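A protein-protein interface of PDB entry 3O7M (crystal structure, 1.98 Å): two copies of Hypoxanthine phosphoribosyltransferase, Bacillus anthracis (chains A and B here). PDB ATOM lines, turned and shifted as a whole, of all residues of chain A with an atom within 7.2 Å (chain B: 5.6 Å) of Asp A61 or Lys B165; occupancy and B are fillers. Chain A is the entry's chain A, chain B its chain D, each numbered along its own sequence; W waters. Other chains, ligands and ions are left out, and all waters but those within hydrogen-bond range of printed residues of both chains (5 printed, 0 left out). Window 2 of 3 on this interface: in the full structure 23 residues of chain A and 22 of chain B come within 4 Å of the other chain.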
ATOM      1  N   GLU A  36      16.916   2.539 -26.727  1.00  0.00           N
ATOM      2  CA  GLU A  36      16.439   3.736 -27.393  1.00  0.00           C
ATOM      3  C   GLU A  36      16.390   4.949 -26.462  1.00  0.00           C
ATOM      4  O   GLU A  36      16.312   4.814 -25.257  1.00  0.00           O
ATOM      5  CB  GLU A  36      15.017   3.505 -27.938  1.00  0.00           C
ATOM      6  CG  GLU A  36      14.866   2.278 -28.828  1.00  0.00           C
ATOM      7  CD  GLU A  36      13.472   2.168 -29.383  1.00  0.00           C
ATOM      8  OE1 GLU A  36      13.118   3.021 -30.242  1.00  0.00           O
ATOM      9  OE2 GLU A  36      12.745   1.257 -28.915  1.00  0.00           O
ATOM     10  N   GLU A  37      16.410   6.128 -27.043  1.00  0.00           N
ATOM     11  CA  GLU A  37      16.224   7.362 -26.279  1.00  0.00           C
ATOM     12  C   GLU A  37      14.756   7.526 -25.978  1.00  0.00           C
ATOM     13  O   GLU A  37      13.899   7.084 -26.731  1.00  0.00           O
ATOM     14  CB  GLU A  37      16.598   8.585 -27.126  1.00  0.00           C
ATOM     15  CG  GLU A  37      17.952   8.514 -27.762  1.00  0.00           C
ATOM     16  CD  GLU A  37      18.310   9.809 -28.490  1.00  0.00           C
ATOM     17  OE1 GLU A  37      17.418  10.446 -29.141  1.00  0.00           O
ATOM     18  OE2 GLU A  37      19.501  10.163 -28.422  1.00  0.00           O
ATOM     19  N   ILE A  38      14.457   8.234 -24.913  1.00  0.00           N
ATOM     20  CA  ILE A  38      13.088   8.505 -24.550  1.00  0.00           C
ATOM     21  C   ILE A  38      12.968   9.973 -24.191  1.00  0.00           C
ATOM     22  O   ILE A  38      13.898  10.573 -23.641  1.00  0.00           O
ATOM     23  CB  ILE A  38      12.679   7.724 -23.313  1.00  0.00           C
ATOM     24  CG1 ILE A  38      12.861   6.204 -23.514  1.00  0.00           C
ATOM     25  CG2 ILE A  38      11.213   8.045 -22.962  1.00  0.00           C
ATOM     26  CD1 ILE A  38      12.861   5.388 -22.150  1.00  0.00           C
ATOM     27  N   VAL A  39      11.837  10.570 -24.537  1.00  0.00           N
ATOM     28  CA  VAL A  39      11.542  11.927 -24.135  1.00  0.00           C
ATOM     29  C   VAL A  39      10.397  11.814 -23.118  1.00  0.00           C
ATOM     30  O   VAL A  39       9.340  11.286 -23.429  1.00  0.00           O
ATOM     31  CB  VAL A  39      11.057  12.849 -25.288  1.00  0.00           C
ATOM     32  CG1 VAL A  39      10.695  14.249 -24.694  1.00  0.00           C
ATOM     33  CG2 VAL A  39      12.119  13.004 -26.386  1.00  0.00           C
ATOM     34  N   ILE A  58      15.175   5.393 -14.591  1.00  0.00           N
ATOM     35  CA  ILE A  58      15.238   5.069 -16.006  1.00  0.00           C
ATOM     36  C   ILE A  58      16.659   5.397 -16.465  1.00  0.00           C
ATOM     37  O   ILE A  58      17.083   6.567 -16.403  1.00  0.00           O
ATOM     38  CB  ILE A  58      14.240   5.904 -16.800  1.00  0.00           C
ATOM     39  CG1 ILE A  58      12.816   5.496 -16.433  1.00  0.00           C
ATOM     40  CG2 ILE A  58      14.480   5.684 -18.336  1.00  0.00           C
ATOM     41  CD1 ILE A  58      11.741   6.483 -17.061  1.00  0.00           C
ATOM     42  N   LYS A  59      17.389   4.390 -16.902  1.00  0.00           N
ATOM     43  CA  LYS A  59      18.767   4.587 -17.318  1.00  0.00           C
ATOM     44  C   LYS A  59      18.980   4.912 -18.772  1.00  0.00           C
ATOM     45  O   LYS A  59      20.101   5.280 -19.152  1.00  0.00           O
ATOM     46  CB  LYS A  59      19.624   3.401 -16.907  1.00  0.00           C
ATOM     47  CG  LYS A  59      19.492   3.088 -15.399  1.00  0.00           C
ATOM     48  CD  LYS A  59      19.626   4.293 -14.486  1.00  0.00           C
ATOM     49  CE  LYS A  59      19.236   3.994 -12.985  1.00  0.00           C
ATOM     50  NZ  LYS A  59      19.370   5.188 -12.057  1.00  0.00           N
ATOM     51  N   ASN A  60      17.934   4.788 -19.589  1.00  0.00           N
ATOM     52  CA  ASN A  60      18.034   5.198 -20.981  1.00  0.00           C
ATOM     53  C   ASN A  60      18.416   6.665 -21.033  1.00  0.00           C
ATOM     54  O   ASN A  60      18.241   7.377 -20.014  1.00  0.00           O
ATOM     55  CB  ASN A  60      16.673   5.101 -21.699  1.00  0.00           C
ATOM     56  CG  ASN A  60      16.119   3.691 -21.708  1.00  0.00           C
ATOM     57  OD1 ASN A  60      16.007   3.064 -20.657  1.00  0.00           O
ATOM     58  ND2 ASN A  60      15.741   3.197 -22.895  1.00  0.00           N
ATOM     59  N   ASP A  61      18.905   7.094 -22.204  1.00  0.00           N
ATOM     60  CA  ASP A  61      19.137   8.524 -22.534  1.00  0.00           C
ATOM     61  C   ASP A  61      17.747   9.093 -22.465  1.00  0.00           C
ATOM     62  O   ASP A  61      16.843   8.675 -23.218  1.00  0.00           O
ATOM     63  CB  ASP A  61      19.710   8.704 -23.956  1.00  0.00           C
ATOM     64  CG  ASP A  61      19.878  10.220 -24.408  1.00  0.00           C
ATOM     65  OD1 ASP A  61      19.230  11.187 -23.892  1.00  0.00           O
ATOM     66  OD2 ASP A  61      20.660  10.441 -25.366  1.00  0.00           O
ATOM     67  N   VAL A  62      17.561  10.017 -21.540  1.00  0.00           N
ATOM     68  CA  VAL A  62      16.253  10.623 -21.306  1.00  0.00           C
ATOM     69  C   VAL A  62      16.338  12.144 -21.490  1.00  0.00           C
ATOM     70  O   VAL A  62      17.324  12.787 -21.080  1.00  0.00           O
ATOM     71  CB  VAL A  62      15.751  10.309 -19.855  1.00  0.00           C
ATOM     72  CG1 VAL A  62      14.631  11.235 -19.441  1.00  0.00           C
ATOM     73  CG2 VAL A  62      15.340   8.839 -19.713  1.00  0.00           C
ATOM     74  N   THR A  63      15.355  12.695 -22.186  1.00  0.00           N
ATOM     75  CA  THR A  63      15.175  14.138 -22.308  1.00  0.00           C
ATOM     76  C   THR A  63      13.882  14.428 -21.533  1.00  0.00           C
ATOM     77  O   THR A  63      12.975  13.618 -21.554  1.00  0.00           O
ATOM     78  CB  THR A  63      15.018  14.543 -23.802  1.00  0.00           C
ATOM     79  OG1 THR A  63      16.277  14.369 -24.450  1.00  0.00           O
ATOM     80  CG2 THR A  63      14.582  15.975 -23.911  1.00  0.00           C
ATOM     81  N   ILE A  64      13.815  15.530 -20.795  1.00  0.00           N
ATOM     82  CA  ILE A  64      12.605  15.881 -20.033  1.00  0.00           C
ATOM     83  C   ILE A  64      12.084  17.237 -20.440  1.00  0.00           C
ATOM     84  O   ILE A  64      12.871  18.139 -20.744  1.00  0.00           O
ATOM     85  CB  ILE A  64      12.935  16.027 -18.517  1.00  0.00           C
ATOM     86  CG1 ILE A  64      13.587  14.790 -17.989  1.00  0.00           C
ATOM     87  CG2 ILE A  64      11.647  16.334 -17.683  1.00  0.00           C
ATOM     88  CD1 ILE A  64      13.930  14.894 -16.533  1.00  0.00           C
ATOM     89  N   ILE B   6      29.372  14.508 -25.558  1.00  0.00           N
ATOM     90  CA  ILE B   6      29.666  14.835 -24.180  1.00  0.00           C
ATOM     91  C   ILE B   6      29.709  13.522 -23.390  1.00  0.00           C
ATOM     92  O   ILE B   6      28.938  12.612 -23.657  1.00  0.00           O
ATOM     93  CB  ILE B   6      28.584  15.767 -23.611  1.00  0.00           C
ATOM     94  CG1 ILE B   6      28.481  17.050 -24.457  1.00  0.00           C
ATOM     95  CG2 ILE B   6      28.857  16.103 -22.149  1.00  0.00           C
ATOM     96  CD1 ILE B   6      29.822  17.767 -24.703  1.00  0.00           C
ATOM     97  N   VAL B 156      26.157  18.072 -14.610  1.00  0.00           N
ATOM     98  CA  VAL B 156      24.879  17.503 -15.012  1.00  0.00           C
ATOM     99  C   VAL B 156      24.384  16.572 -13.938  1.00  0.00           C
ATOM    100  O   VAL B 156      25.135  16.155 -13.029  1.00  0.00           O
ATOM    101  CB  VAL B 156      24.978  16.669 -16.291  1.00  0.00           C
ATOM    102  CG1 VAL B 156      25.476  17.496 -17.445  1.00  0.00           C
ATOM    103  CG2 VAL B 156      25.854  15.423 -16.017  1.00  0.00           C
ATOM    104  N   ILE B 160      19.684  18.655 -13.664  1.00  0.00           N
ATOM    105  CA  ILE B 160      20.523  19.581 -14.444  1.00  0.00           C
ATOM    106  C   ILE B 160      20.983  18.946 -15.762  1.00  0.00           C
ATOM    107  O   ILE B 160      21.463  17.823 -15.785  1.00  0.00           O
ATOM    108  CB  ILE B 160      21.739  20.009 -13.584  1.00  0.00           C
ATOM    109  CG1 ILE B 160      21.288  20.581 -12.231  1.00  0.00           C
ATOM    110  CG2 ILE B 160      22.631  20.981 -14.325  1.00  0.00           C
ATOM    111  CD1 ILE B 160      22.476  20.738 -11.154  1.00  0.00           C
ATOM    112  N   ASP B 161      20.837  19.659 -16.877  1.00  0.00           N
ATOM    113  CA  ASP B 161      21.186  19.102 -18.174  1.00  0.00           C
ATOM    114  C   ASP B 161      22.451  19.650 -18.784  1.00  0.00           C
ATOM    115  O   ASP B 161      23.002  20.650 -18.334  1.00  0.00           O
ATOM    116  CB  ASP B 161      20.091  19.424 -19.194  1.00  0.00           C
ATOM    117  CG  ASP B 161      20.057  20.922 -19.565  1.00  0.00           C
ATOM    118  OD1 ASP B 161      20.048  21.756 -18.649  1.00  0.00           O
ATOM    119  OD2 ASP B 161      20.083  21.236 -20.773  1.00  0.00           O
ATOM    120  N   CYS B 162      22.905  18.941 -19.803  1.00  0.00           N
ATOM    121  CA  CYS B 162      23.910  19.455 -20.753  1.00  0.00           C
ATOM    122  C   CYS B 162      23.225  19.213 -22.077  1.00  0.00           C
ATOM    123  O   CYS B 162      23.004  18.073 -22.464  1.00  0.00           O
ATOM    124  CB  CYS B 162      25.240  18.741 -20.703  1.00  0.00           C
ATOM    125  SG  CYS B 162      26.316  19.217 -22.089  1.00  0.00           S
ATOM    126  N   ALA B 163      22.812  20.283 -22.740  1.00  0.00           N
ATOM    127  CA  ALA B 163      22.059  20.170 -23.998  1.00  0.00           C
ATOM    128  C   ALA B 163      20.914  19.144 -23.915  1.00  0.00           C
ATOM    129  O   ALA B 163      20.774  18.247 -24.763  1.00  0.00           O
ATOM    130  CB  ALA B 163      22.981  19.866 -25.167  1.00  0.00           C
ATOM    131  N   GLU B 164      20.121  19.302 -22.858  1.00  0.00           N
ATOM    132  CA  GLU B 164      18.924  18.507 -22.556  1.00  0.00           C
ATOM    133  C   GLU B 164      19.170  17.088 -22.035  1.00  0.00           C
ATOM    134  O   GLU B 164      18.212  16.408 -21.633  1.00  0.00           O
ATOM    135  CB  GLU B 164      17.930  18.483 -23.715  1.00  0.00           C
ATOM    136  CG  GLU B 164      17.357  19.866 -24.075  1.00  0.00           C
ATOM    137  CD  GLU B 164      16.600  20.557 -22.953  1.00  0.00           C
ATOM    138  OE1 GLU B 164      15.998  19.897 -22.061  1.00  0.00           O
ATOM    139  OE2 GLU B 164      16.584  21.808 -22.974  1.00  0.00           O
ATOM    140  N   LYS B 165      20.436  16.682 -21.994  1.00  0.00           N
ATOM    141  CA  LYS B 165      20.827  15.346 -21.557  1.00  0.00           C
ATOM    142  C   LYS B 165      21.260  15.302 -20.096  1.00  0.00           C
ATOM    143  O   LYS B 165      21.631  16.318 -19.507  1.00  0.00           O
ATOM    144  CB  LYS B 165      21.986  14.855 -22.422  1.00  0.00           C
ATOM    145  CG  LYS B 165      22.293  13.367 -22.306  1.00  0.00           C
ATOM    146  CD  LYS B 165      23.330  12.979 -23.337  1.00  0.00           C
ATOM    147  CE  LYS B 165      23.674  11.513 -23.335  1.00  0.00           C
ATOM    148  NZ  LYS B 165      24.719  11.286 -24.399  1.00  0.00           N
ATOM    149  N   TYR B 166      21.160  14.103 -19.524  1.00  0.00           N
ATOM    150  CA  TYR B 166      21.601  13.783 -18.181  1.00  0.00           C
ATOM    151  C   TYR B 166      20.811  14.253 -16.977  1.00  0.00           C
ATOM    152  O   TYR B 166      21.278  14.089 -15.851  1.00  0.00           O
ATOM    153  CB  TYR B 166      23.091  14.114 -17.978  1.00  0.00           C
ATOM    154  CG  TYR B 166      24.008  13.380 -18.900  1.00  0.00           C
ATOM    155  CD1 TYR B 166      24.689  14.047 -19.910  1.00  0.00           C
ATOM    156  CD2 TYR B 166      24.187  12.010 -18.777  1.00  0.00           C
ATOM    157  CE1 TYR B 166      25.549  13.370 -20.759  1.00  0.00           C
ATOM    158  CE2 TYR B 166      25.047  11.332 -19.611  1.00  0.00           C
ATOM    159  CZ  TYR B 166      25.727  12.012 -20.581  1.00  0.00           C
ATOM    160  OH  TYR B 166      26.558  11.317 -21.413  1.00  0.00           O
ATOM    161  N   ARG B 167      19.629  14.807 -17.188  1.00  0.00           N
ATOM    162  CA  ARG B 167      18.844  15.269 -16.048  1.00  0.00           C
ATOM    163  C   ARG B 167      18.383  14.126 -15.181  1.00  0.00           C
ATOM    164  O   ARG B 167      18.092  14.330 -13.987  1.00  0.00           O
ATOM    165  CB  ARG B 167      17.605  16.042 -16.501  1.00  0.00           C
ATOM    166  CG  ARG B 167      17.815  17.315 -17.272  1.00  0.00           C
ATOM    167  CD  ARG B 167      16.414  17.918 -17.512  1.00  0.00           C
ATOM    168  NE  ARG B 167      16.381  19.031 -18.453  1.00  0.00           N
ATOM    169  CZ  ARG B 167      16.676  20.305 -18.183  1.00  0.00           C
ATOM    170  NH1 ARG B 167      17.077  20.730 -16.987  1.00  0.00           N
ATOM    171  NH2 ARG B 167      16.553  21.183 -19.139  1.00  0.00           N
ATOM    172  N   ASN B 168      18.361  12.916 -15.747  1.00  0.00           N
ATOM    173  CA  ASN B 168      17.922  11.718 -15.046  1.00  0.00           C
ATOM    174  C   ASN B 168      18.950  11.021 -14.138  1.00  0.00           C
ATOM    175  O   ASN B 168      18.588  10.062 -13.432  1.00  0.00           O
ATOM    176  CB  ASN B 168      17.351  10.685 -16.038  1.00  0.00           C
ATOM    177  CG  ASN B 168      18.349  10.291 -17.097  1.00  0.00           C
ATOM    178  OD1 ASN B 168      19.083  11.146 -17.573  1.00  0.00           O
ATOM    179  ND2 ASN B 168      18.415   9.005 -17.449  1.00  0.00           N
HETATM  180  O   HOH W   1      13.552  20.615 -21.434  1.00  0.00           O
HETATM  181  O   HOH W   2      15.957  17.536 -20.869  1.00  0.00           O
HETATM  182  O   HOH W   3      18.448   7.500 -13.956  1.00  0.00           O
HETATM  183  O   HOH W   4      19.996  11.514 -20.419  1.00  0.00           O
HETATM  184  O   HOH W   5      17.927  14.822 -19.519  1.00  0.00           O
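The side-chain amide nitrogen of Asn A60 is in hydrogen-bond range of the backbone carbonyl oxygen of Glu A36, at 2.9 Å. The backbone NH of Ile A38 is in hydrogen-bond range of the backbone carbonyl oxygen of Asp A61, at 3.0 Å. The backbone carbonyl oxygen of Ile A38 lies within hydrogen-bond range of the backbone NH of Thr A63 (3.0 Å). OD2 of Asp B161 is in hydrogen-bond range of N of Glu B164, 2.8 Å away. NH1 of Arg B167 lies within salt-bridge range of OD1 of Asp B161 (3.6 Å). The side-chain carboxylate (OE1) of Glu B164 lies within salt-bridge range of the guanidinium group (NH2) of Arg B167 (3.2 Å).
O of Ile A58 is in hydrogen-bond range of ND2 of Asn B168, 3.0 Å away. O of Asn A60 lies within hydrogen-bond range of ND2 of Asn B168, at 3.0 Å.
OD2 of Asp A61 touches CE of Lys B165, 3.8 Å away. Glu B164 touches Val A62 (O to O, 3.8 Å). Val A62 touches Asn B168 (CB to CG, 3.8 Å). O of Glu B164 touches CA of Thr A63, at 3.9 Å. OE1 of Glu B164 touches O of Ile A64, at 3.8 Å. CD1 of Ile A64 touches CB of Arg B167, 3.9 Å away.
Printed residues of chain B that touch a printed residue of chain A: Glu B164, Lys B165, Arg B167 and Asn B168. Among the printed residues, 8 pairs touch across the chains. Among the printed residues, no Asp or Glu carboxylate lies within 4 Å of a Lys or Arg side-chain nitrogen of the other chain.
Water W3 lies within hydrogen-bond range of O of Asn B168, O of Ile A58 and NZ of Lys A59. Water W1 bridges OE1 of Glu B164 (2.6 Å) and O of Ile A64 (2.7 Å). Water W2 lies within hydrogen-bond range of the backbone carbonyl oxygen (O) of Glu B164 (2.6 Å), the guanidinium group (NE) of Arg B167 (2.9 Å) and the backbone NH (N) of Ile A64 (2.9 Å). Water W5 lies within hydrogen-bond range of the backbone carbonyl oxygen (O) of Val A62, the backbone carbonyl oxygen (O) of Glu B164, the backbone NH (N) of Arg B167 and the backbone NH (N) of Tyr B166. Water W4 lies within hydrogen-bond range of N of Tyr B166 (3.0 Å), OD1 of Asn B168 (3.0 Å) and O of Val A62 (3.0 Å).
Of the printed residues of chain B, Asn A60 touches Asn B168. Of the printed residues of chain B, Ile A64 touches Glu B164 and Arg B167. Ile B6 touches none of the printed residues of chain A. Printed residues of chain A within 4 Å of Lys B165: Asp A61. Of the printed residues of chain A, Arg B167 touches Ile A64 (3.9 Å). Of the printed residues of chain A, Asn B168 touches Ile A58, Asn A60 and Val A62. The nearest printed residue of chain A that does not touch Lys B165 is Val A62 (4.4 Å). The nearest printed residue of chain B that does not touch Asn A60 is Tyr B166 (7.3 Å).
No position is printed for both chains. Of the 8 pairs that touch across the chains among the printed residues, none has its exchanged pair printed and touching as well.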
